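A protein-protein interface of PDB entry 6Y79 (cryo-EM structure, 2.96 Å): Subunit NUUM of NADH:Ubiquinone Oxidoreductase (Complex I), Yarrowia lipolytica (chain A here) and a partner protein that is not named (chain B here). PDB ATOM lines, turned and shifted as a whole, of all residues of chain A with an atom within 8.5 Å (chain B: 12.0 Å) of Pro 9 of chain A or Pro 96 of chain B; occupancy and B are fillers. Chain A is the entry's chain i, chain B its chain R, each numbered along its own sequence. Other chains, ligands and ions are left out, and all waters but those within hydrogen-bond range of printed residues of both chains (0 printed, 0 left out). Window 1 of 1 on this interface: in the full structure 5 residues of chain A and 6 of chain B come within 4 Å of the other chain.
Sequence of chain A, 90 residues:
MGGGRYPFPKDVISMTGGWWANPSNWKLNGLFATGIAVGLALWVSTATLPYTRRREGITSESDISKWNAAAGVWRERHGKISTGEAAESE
Among the printed residues, pairs that only touch across the chains: Tyr 6 of chain A with Asn 93 of chain B (3.5 Å), Tyr 6 of chain A with Pro 95 of chain B (3.7 Å), Pro 7 of chain A with Met 98 of chain B (3.4 Å), Phe 8 of chain A with Met 98 of chain B (3.7 Å), Pro 9 of chain A with Pro 96 of chain B (3.8 Å), Asp 11 of chain A with Glu 99 of chain B (3.7 Å) and Asp 11 of chain A with Ile 101 of chain B (3.7 Å).
Printed residues of chain B within 4 Å of Tyr 6 of chain A: Asn 93 (3.5 Å) and Pro 95 (3.7 Å).
Pro 7 of chain A touches one residue of chain B.
Of chain B, only Met 98 (3.7 Å) comes within 4 Å of Phe 8 of chain A.
Pro 9 of chain A touches just one residue of chain B: Pro 96 (3.8 Å).
Printed residues of chain B within 4 Å of Asp 11 of chain A: Glu 99 (3.7 Å) and Ile 101 (3.7 Å).
No residue of chain B comes within 4 Å of Val 12 of chain A.
Printed residues of chain A within 4 Å of Asn 93 of chain B: Tyr 6 (3.5 Å).
Printed residues of chain A within 4 Å of Pro 96 of chain B: Pro 9.
Printed residues of chain A within 4 Å of Met 98 of chain B: Pro 7 and Phe 8.
Printed residues of chain A within 4 Å of Ile 101 of chain B: Asp 11 (3.7 Å).
The nearest printed residue of chain A that does not touch Pro 96 of chain B is Trp 19 of chain A (4.02 Å).
Along chain B the printed residues that touch a printed residue of chain A span positions 93 to 101.
Along chain A the printed residues that touch a printed residue of chain B span positions 6 to 11.
Among the printed residues, 7 pairs touch across the chains.
Among the printed residues, no Asp or Glu carboxylate lies within 4 Å of a Lys or Arg side-chain nitrogen of the other chain.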
ATOM      1  N   TYR A   6     -19.861  13.382 -25.454  1.00  0.00           N
ATOM      2  CA  TYR A   6     -20.985  12.574 -24.995  1.00  0.00           C
ATOM      3  C   TYR A   6     -22.157  12.630 -25.983  1.00  0.00           C
ATOM      4  O   TYR A   6     -22.303  13.604 -26.724  1.00  0.00           O
ATOM      5  CB  TYR A   6     -21.437  13.055 -23.613  1.00  0.00           C
ATOM      6  CG  TYR A   6     -21.789  14.527 -23.523  1.00  0.00           C
ATOM      7  CD1 TYR A   6     -23.090  14.964 -23.740  1.00  0.00           C
ATOM      8  CD2 TYR A   6     -20.828  15.475 -23.193  1.00  0.00           C
ATOM      9  CE1 TYR A   6     -23.415  16.291 -23.656  1.00  0.00           C
ATOM     10  CE2 TYR A   6     -21.148  16.810 -23.106  1.00  0.00           C
ATOM     11  CZ  TYR A   6     -22.443  17.209 -23.338  1.00  0.00           C
ATOM     12  OH  TYR A   6     -22.776  18.537 -23.250  1.00  0.00           O
ATOM     13  N   PRO A   7     -22.992  11.590 -26.034  1.00  0.00           N
ATOM     14  CA  PRO A   7     -24.122  11.612 -26.970  1.00  0.00           C
ATOM     15  C   PRO A   7     -25.259  12.496 -26.481  1.00  0.00           C
ATOM     16  O   PRO A   7     -25.495  12.647 -25.282  1.00  0.00           O
ATOM     17  CB  PRO A   7     -24.553  10.144 -27.035  1.00  0.00           C
ATOM     18  CG  PRO A   7     -24.127   9.582 -25.736  1.00  0.00           C
ATOM     19  CD  PRO A   7     -22.836  10.261 -25.413  1.00  0.00           C
ATOM     20  N   PHE A   8     -25.982  13.065 -27.436  1.00  0.00           N
ATOM     21  CA  PHE A   8     -27.060  14.009 -27.191  1.00  0.00           C
ATOM     22  C   PHE A   8     -28.299  13.585 -27.963  1.00  0.00           C
ATOM     23  O   PHE A   8     -28.200  12.865 -28.961  1.00  0.00           O
ATOM     24  CB  PHE A   8     -26.644  15.439 -27.586  1.00  0.00           C
ATOM     25  CG  PHE A   8     -26.298  15.616 -29.042  1.00  0.00           C
ATOM     26  CD1 PHE A   8     -25.009  15.400 -29.489  1.00  0.00           C
ATOM     27  CD2 PHE A   8     -27.250  16.050 -29.953  1.00  0.00           C
ATOM     28  CE1 PHE A   8     -24.684  15.574 -30.821  1.00  0.00           C
ATOM     29  CE2 PHE A   8     -26.933  16.223 -31.286  1.00  0.00           C
ATOM     30  CZ  PHE A   8     -25.649  15.987 -31.719  1.00  0.00           C
ATOM     31  N   PRO A   9     -29.489  14.002 -27.522  1.00  0.00           N
ATOM     32  CA  PRO A   9     -30.695  13.740 -28.320  1.00  0.00           C
ATOM     33  C   PRO A   9     -30.811  14.719 -29.479  1.00  0.00           C
ATOM     34  O   PRO A   9     -30.664  15.929 -29.302  1.00  0.00           O
ATOM     35  CB  PRO A   9     -31.838  13.923 -27.312  1.00  0.00           C
ATOM     36  CG  PRO A   9     -31.288  14.824 -26.278  1.00  0.00           C
ATOM     37  CD  PRO A   9     -29.830  14.495 -26.172  1.00  0.00           C
ATOM     38  N   LYS A  10     -31.073  14.186 -30.668  1.00  0.00           N
ATOM     39  CA  LYS A  10     -31.315  14.993 -31.853  1.00  0.00           C
ATOM     40  C   LYS A  10     -32.781  15.362 -32.008  1.00  0.00           C
ATOM     41  O   LYS A  10     -33.127  16.013 -33.008  1.00  0.00           O
ATOM     42  CB  LYS A  10     -30.805  14.244 -33.092  1.00  0.00           C
ATOM     43  CG  LYS A  10     -29.362  13.804 -32.977  1.00  0.00           C
ATOM     44  CD  LYS A  10     -28.861  13.184 -34.260  1.00  0.00           C
ATOM     45  CE  LYS A  10     -27.379  12.866 -34.171  1.00  0.00           C
ATOM     46  NZ  LYS A  10     -26.872  12.215 -35.411  1.00  0.00           N
ATOM     47  N   ASP A  11     -33.617  14.940 -31.037  1.00  0.00           N
ATOM     48  CA  ASP A  11     -35.018  15.327 -30.946  1.00  0.00           C
ATOM     49  C   ASP A  11     -35.200  16.833 -31.031  1.00  0.00           C
ATOM     50  O   ASP A  11     -36.081  17.322 -31.746  1.00  0.00           O
ATOM     51  CB  ASP A  11     -35.573  14.894 -29.606  1.00  0.00           C
ATOM     52  CG  ASP A  11     -36.271  13.557 -29.631  1.00  0.00           C
ATOM     53  OD1 ASP A  11     -36.601  13.014 -30.707  1.00  0.00           O
ATOM     54  OD2 ASP A  11     -36.486  13.049 -28.508  1.00  0.00           O
ATOM     55  N   VAL A  12     -34.407  17.560 -30.280  1.00  0.00           N
ATOM     56  CA  VAL A  12     -34.756  18.896 -29.837  1.00  0.00           C
ATOM     57  C   VAL A  12     -34.091  19.924 -30.742  1.00  0.00           C
ATOM     58  O   VAL A  12     -32.992  19.718 -31.274  1.00  0.00           O
ATOM     59  CB  VAL A  12     -34.383  19.042 -28.347  1.00  0.00           C
ATOM     60  CG1 VAL A  12     -32.925  18.983 -28.139  1.00  0.00           C
ATOM     61  CG2 VAL A  12     -34.961  20.290 -27.759  1.00  0.00           C
ATOM     62  N   ILE A  13     -34.793  21.025 -30.967  1.00  0.00           N
ATOM     63  CA  ILE A  13     -34.371  22.055 -31.900  1.00  0.00           C
ATOM     64  C   ILE A  13     -34.303  23.367 -31.141  1.00  0.00           C
ATOM     65  O   ILE A  13     -35.315  23.826 -30.601  1.00  0.00           O
ATOM     66  CB  ILE A  13     -35.326  22.173 -33.102  1.00  0.00           C
ATOM     67  CG1 ILE A  13     -35.302  20.888 -33.925  1.00  0.00           C
ATOM     68  CG2 ILE A  13     -34.972  23.367 -33.955  1.00  0.00           C
ATOM     69  CD1 ILE A  13     -36.403  20.816 -34.952  1.00  0.00           C
ATOM     70  N   GLY A  17     -28.659  26.587 -31.852  1.00  0.00           N
ATOM     71  CA  GLY A  17     -27.956  25.502 -32.499  1.00  0.00           C
ATOM     72  C   GLY A  17     -28.139  24.124 -31.908  1.00  0.00           C
ATOM     73  O   GLY A  17     -28.306  23.152 -32.647  1.00  0.00           O
ATOM     74  N   GLY A  18     -28.138  24.021 -30.589  1.00  0.00           N
ATOM     75  CA  GLY A  18     -28.082  22.719 -29.962  1.00  0.00           C
ATOM     76  C   GLY A  18     -26.700  22.472 -29.408  1.00  0.00           C
ATOM     77  O   GLY A  18     -26.005  23.429 -29.061  1.00  0.00           O
ATOM     78  N   TRP A  19     -26.265  21.212 -29.337  1.00  0.00           N
ATOM     79  CA  TRP A  19     -25.015  20.934 -28.631  1.00  0.00           C
ATOM     80  C   TRP A  19     -23.790  21.243 -29.482  1.00  0.00           C
ATOM     81  O   TRP A  19     -23.088  22.216 -29.224  1.00  0.00           O
ATOM     82  CB  TRP A  19     -24.983  19.486 -28.148  1.00  0.00           C
ATOM     83  CG  TRP A  19     -25.839  19.267 -26.977  1.00  0.00           C
ATOM     84  CD1 TRP A  19     -25.470  19.280 -25.671  1.00  0.00           C
ATOM     85  CD2 TRP A  19     -27.231  19.004 -27.002  1.00  0.00           C
ATOM     86  NE1 TRP A  19     -26.557  19.039 -24.874  1.00  0.00           N
ATOM     87  CE2 TRP A  19     -27.654  18.865 -25.672  1.00  0.00           C
ATOM     88  CE3 TRP A  19     -28.163  18.867 -28.025  1.00  0.00           C
ATOM     89  CZ2 TRP A  19     -28.967  18.595 -25.340  1.00  0.00           C
ATOM     90  CZ3 TRP A  19     -29.450  18.600 -27.699  1.00  0.00           C
ATOM     91  CH2 TRP A  19     -29.850  18.466 -26.367  1.00  0.00           C
ATOM     92  N   TRP A  20     -23.554  20.484 -30.542  1.00  0.00           N
ATOM     93  CA  TRP A  20     -22.332  20.718 -31.304  1.00  0.00           C
ATOM     94  C   TRP A  20     -22.670  21.099 -32.733  1.00  0.00           C
ATOM     95  O   TRP A  20     -22.113  20.521 -33.669  1.00  0.00           O
ATOM     96  CB  TRP A  20     -21.421  19.488 -31.300  1.00  0.00           C
ATOM     97  CG  TRP A  20     -20.684  19.216 -30.018  1.00  0.00           C
ATOM     98  CD1 TRP A  20     -19.507  19.764 -29.616  1.00  0.00           C
ATOM     99  CD2 TRP A  20     -21.068  18.296 -28.993  1.00  0.00           C
ATOM    100  NE1 TRP A  20     -19.141  19.254 -28.398  1.00  0.00           N
ATOM    101  CE2 TRP A  20     -20.086  18.351 -27.994  1.00  0.00           C
ATOM    102  CE3 TRP A  20     -22.151  17.435 -28.825  1.00  0.00           C
ATOM    103  CZ2 TRP A  20     -20.158  17.585 -26.843  1.00  0.00           C
ATOM    104  CZ3 TRP A  20     -22.224  16.683 -27.682  1.00  0.00           C
ATOM    105  CH2 TRP A  20     -21.234  16.759 -26.705  1.00  0.00           C
ATOM    106  N   GLU B  91     -20.045  19.078 -12.621  1.00  0.00           N
ATOM    107  CA  GLU B  91     -21.311  19.294 -13.332  1.00  0.00           C
ATOM    108  C   GLU B  91     -21.221  20.437 -14.336  1.00  0.00           C
ATOM    109  O   GLU B  91     -22.055  21.339 -14.352  1.00  0.00           O
ATOM    110  CB  GLU B  91     -22.469  19.524 -12.363  1.00  0.00           C
ATOM    111  CG  GLU B  91     -22.752  18.374 -11.451  1.00  0.00           C
ATOM    112  CD  GLU B  91     -23.827  18.701 -10.444  1.00  0.00           C
ATOM    113  OE1 GLU B  91     -24.211  19.885 -10.344  1.00  0.00           O
ATOM    114  OE2 GLU B  91     -24.292  17.773  -9.749  1.00  0.00           O
ATOM    115  N   ARG B  92     -20.206  20.397 -15.193  1.00  0.00           N
ATOM    116  CA  ARG B  92     -20.163  21.385 -16.261  1.00  0.00           C
ATOM    117  C   ARG B  92     -21.082  20.986 -17.408  1.00  0.00           C
ATOM    118  O   ARG B  92     -22.046  21.693 -17.718  1.00  0.00           O
ATOM    119  CB  ARG B  92     -18.732  21.591 -16.742  1.00  0.00           C
ATOM    120  CG  ARG B  92     -18.014  22.629 -15.931  1.00  0.00           C
ATOM    121  CD  ARG B  92     -16.572  22.735 -16.325  1.00  0.00           C
ATOM    122  NE  ARG B  92     -16.390  23.491 -17.551  1.00  0.00           N
ATOM    123  CZ  ARG B  92     -15.233  23.588 -18.189  1.00  0.00           C
ATOM    124  NH1 ARG B  92     -14.173  22.966 -17.715  1.00  0.00           N
ATOM    125  NH2 ARG B  92     -15.129  24.294 -19.301  1.00  0.00           N
ATOM    126  N   ASN B  93     -20.822  19.846 -18.033  1.00  0.00           N
ATOM    127  CA  ASN B  93     -21.695  19.338 -19.084  1.00  0.00           C
ATOM    128  C   ASN B  93     -22.160  17.951 -18.675  1.00  0.00           C
ATOM    129  O   ASN B  93     -21.592  16.937 -19.083  1.00  0.00           O
ATOM    130  CB  ASN B  93     -20.997  19.340 -20.388  1.00  0.00           C
ATOM    131  CG  ASN B  93     -20.850  20.732 -20.954  1.00  0.00           C
ATOM    132  OD1 ASN B  93     -19.762  21.149 -21.335  1.00  0.00           O
ATOM    133  ND2 ASN B  93     -21.956  21.464 -21.007  1.00  0.00           N
ATOM    134  N   VAL B  94     -23.201  17.920 -17.853  1.00  0.00           N
ATOM    135  CA  VAL B  94     -23.889  16.690 -17.497  1.00  0.00           C
ATOM    136  C   VAL B  94     -24.570  16.196 -18.763  1.00  0.00           C
ATOM    137  O   VAL B  94     -25.350  16.949 -19.362  1.00  0.00           O
ATOM    138  CB  VAL B  94     -24.898  16.926 -16.366  1.00  0.00           C
ATOM    139  CG1 VAL B  94     -25.784  15.709 -16.175  1.00  0.00           C
ATOM    140  CG2 VAL B  94     -24.171  17.284 -15.087  1.00  0.00           C
ATOM    141  N   PRO B  95     -24.277  14.988 -19.236  1.00  0.00           N
ATOM    142  CA  PRO B  95     -24.950  14.480 -20.422  1.00  0.00           C
ATOM    143  C   PRO B  95     -26.410  14.206 -20.126  1.00  0.00           C
ATOM    144  O   PRO B  95     -26.735  13.594 -19.098  1.00  0.00           O
ATOM    145  CB  PRO B  95     -24.187  13.185 -20.732  1.00  0.00           C
ATOM    146  CG  PRO B  95     -22.897  13.319 -20.023  1.00  0.00           C
ATOM    147  CD  PRO B  95     -23.219  14.074 -18.782  1.00  0.00           C
ATOM    148  N   PRO B  96     -27.318  14.684 -20.973  1.00  0.00           N
ATOM    149  CA  PRO B  96     -28.740  14.429 -20.740  1.00  0.00           C
ATOM    150  C   PRO B  96     -29.065  12.963 -20.957  1.00  0.00           C
ATOM    151  O   PRO B  96     -28.480  12.303 -21.818  1.00  0.00           O
ATOM    152  CB  PRO B  96     -29.431  15.316 -21.778  1.00  0.00           C
ATOM    153  CG  PRO B  96     -28.420  15.496 -22.842  1.00  0.00           C
ATOM    154  CD  PRO B  96     -27.091  15.503 -22.173  1.00  0.00           C
ATOM    155  N   ARG B  97     -29.980  12.445 -20.147  1.00  0.00           N
ATOM    156  CA  ARG B  97     -30.357  11.050 -20.289  1.00  0.00           C
ATOM    157  C   ARG B  97     -31.202  10.872 -21.546  1.00  0.00           C
ATOM    158  O   ARG B  97     -31.906  11.789 -21.976  1.00  0.00           O
ATOM    159  CB  ARG B  97     -31.098  10.568 -19.043  1.00  0.00           C
ATOM    160  CG  ARG B  97     -32.475  11.141 -18.850  1.00  0.00           C
ATOM    161  CD  ARG B  97     -33.028  10.776 -17.492  1.00  0.00           C
ATOM    162  NE  ARG B  97     -32.256  11.382 -16.414  1.00  0.00           N
ATOM    163  CZ  ARG B  97     -32.456  12.611 -15.950  1.00  0.00           C
ATOM    164  NH1 ARG B  97     -33.398  13.381 -16.469  1.00  0.00           N
ATOM    165  NH2 ARG B  97     -31.706  13.072 -14.961  1.00  0.00           N
ATOM    166  N   MET B  98     -31.081   9.706 -22.169  1.00  0.00           N
ATOM    167  CA  MET B  98     -31.771   9.458 -23.429  1.00  0.00           C
ATOM    168  C   MET B  98     -33.243   9.204 -23.153  1.00  0.00           C
ATOM    169  O   MET B  98     -33.607   8.188 -22.554  1.00  0.00           O
ATOM    170  CB  MET B  98     -31.137   8.284 -24.165  1.00  0.00           C
ATOM    171  CG  MET B  98     -29.785   8.623 -24.747  1.00  0.00           C
ATOM    172  SD  MET B  98     -29.835  10.223 -25.569  1.00  0.00           S
ATOM    173  CE  MET B  98     -28.095  10.500 -25.814  1.00  0.00           C
ATOM    174  N   GLU B  99     -34.090  10.130 -23.585  1.00  0.00           N
ATOM    175  CA  GLU B  99     -35.515  10.071 -23.311  1.00  0.00           C
ATOM    176  C   GLU B  99     -36.282  10.416 -24.569  1.00  0.00           C
ATOM    177  O   GLU B  99     -36.000  11.430 -25.211  1.00  0.00           O
ATOM    178  CB  GLU B  99     -35.901  11.032 -22.192  1.00  0.00           C
ATOM    179  CG  GLU B  99     -35.634  10.511 -20.807  1.00  0.00           C
ATOM    180  CD  GLU B  99     -36.042  11.502 -19.746  1.00  0.00           C
ATOM    181  OE1 GLU B  99     -36.214  12.686 -20.090  1.00  0.00           O
ATOM    182  OE2 GLU B  99     -36.199  11.105 -18.576  1.00  0.00           O
ATOM    183  N   LYS B 100     -37.244   9.575 -24.922  1.00  0.00           N
ATOM    184  CA  LYS B 100     -38.143   9.937 -25.997  1.00  0.00           C
ATOM    185  C   LYS B 100     -39.249  10.831 -25.449  1.00  0.00           C
ATOM    186  O   LYS B 100     -39.496  10.891 -24.245  1.00  0.00           O
ATOM    187  CB  LYS B 100     -38.723   8.691 -26.670  1.00  0.00           C
ATOM    188  CG  LYS B 100     -37.894   8.152 -27.839  1.00  0.00           C
ATOM    189  CD  LYS B 100     -36.686   7.356 -27.362  1.00  0.00           C
ATOM    190  CE  LYS B 100     -37.108   6.073 -26.672  1.00  0.00           C
ATOM    191  NZ  LYS B 100     -35.942   5.336 -26.113  1.00  0.00           N
ATOM    192  N   ILE B 101     -39.918  11.531 -26.355  1.00  0.00           N
ATOM    193  CA  ILE B 101     -40.841  12.591 -25.974  1.00  0.00           C
ATOM    194  C   ILE B 101     -42.159  11.986 -25.508  1.00  0.00           C
ATOM    195  O   ILE B 101     -42.829  11.274 -26.261  1.00  0.00           O
ATOM    196  CB  ILE B 101     -41.067  13.556 -27.140  1.00  0.00           C
ATOM    197  CG1 ILE B 101     -39.772  14.275 -27.491  1.00  0.00           C
ATOM    198  CG2 ILE B 101     -42.127  14.547 -26.793  1.00  0.00           C
ATOM    199  CD1 ILE B 101     -39.865  15.078 -28.753  1.00  0.00           C
ATOM    200  N   MET B 102     -42.531  12.270 -24.264  1.00  0.00           N
ATOM    201  CA  MET B 102     -43.864  11.962 -23.771  1.00  0.00           C
ATOM    202  C   MET B 102     -44.832  13.013 -24.287  1.00  0.00           C
ATOM    203  O   MET B 102     -44.483  14.188 -24.393  1.00  0.00           O
ATOM    204  CB  MET B 102     -43.866  11.936 -22.244  1.00  0.00           C
ATOM    205  CG  MET B 102     -45.165  11.545 -21.597  1.00  0.00           C
ATOM    206  SD  MET B 102     -45.401   9.776 -21.669  1.00  0.00           S
ATOM    207  CE  MET B 102     -44.025   9.245 -20.664  1.00  0.00           C
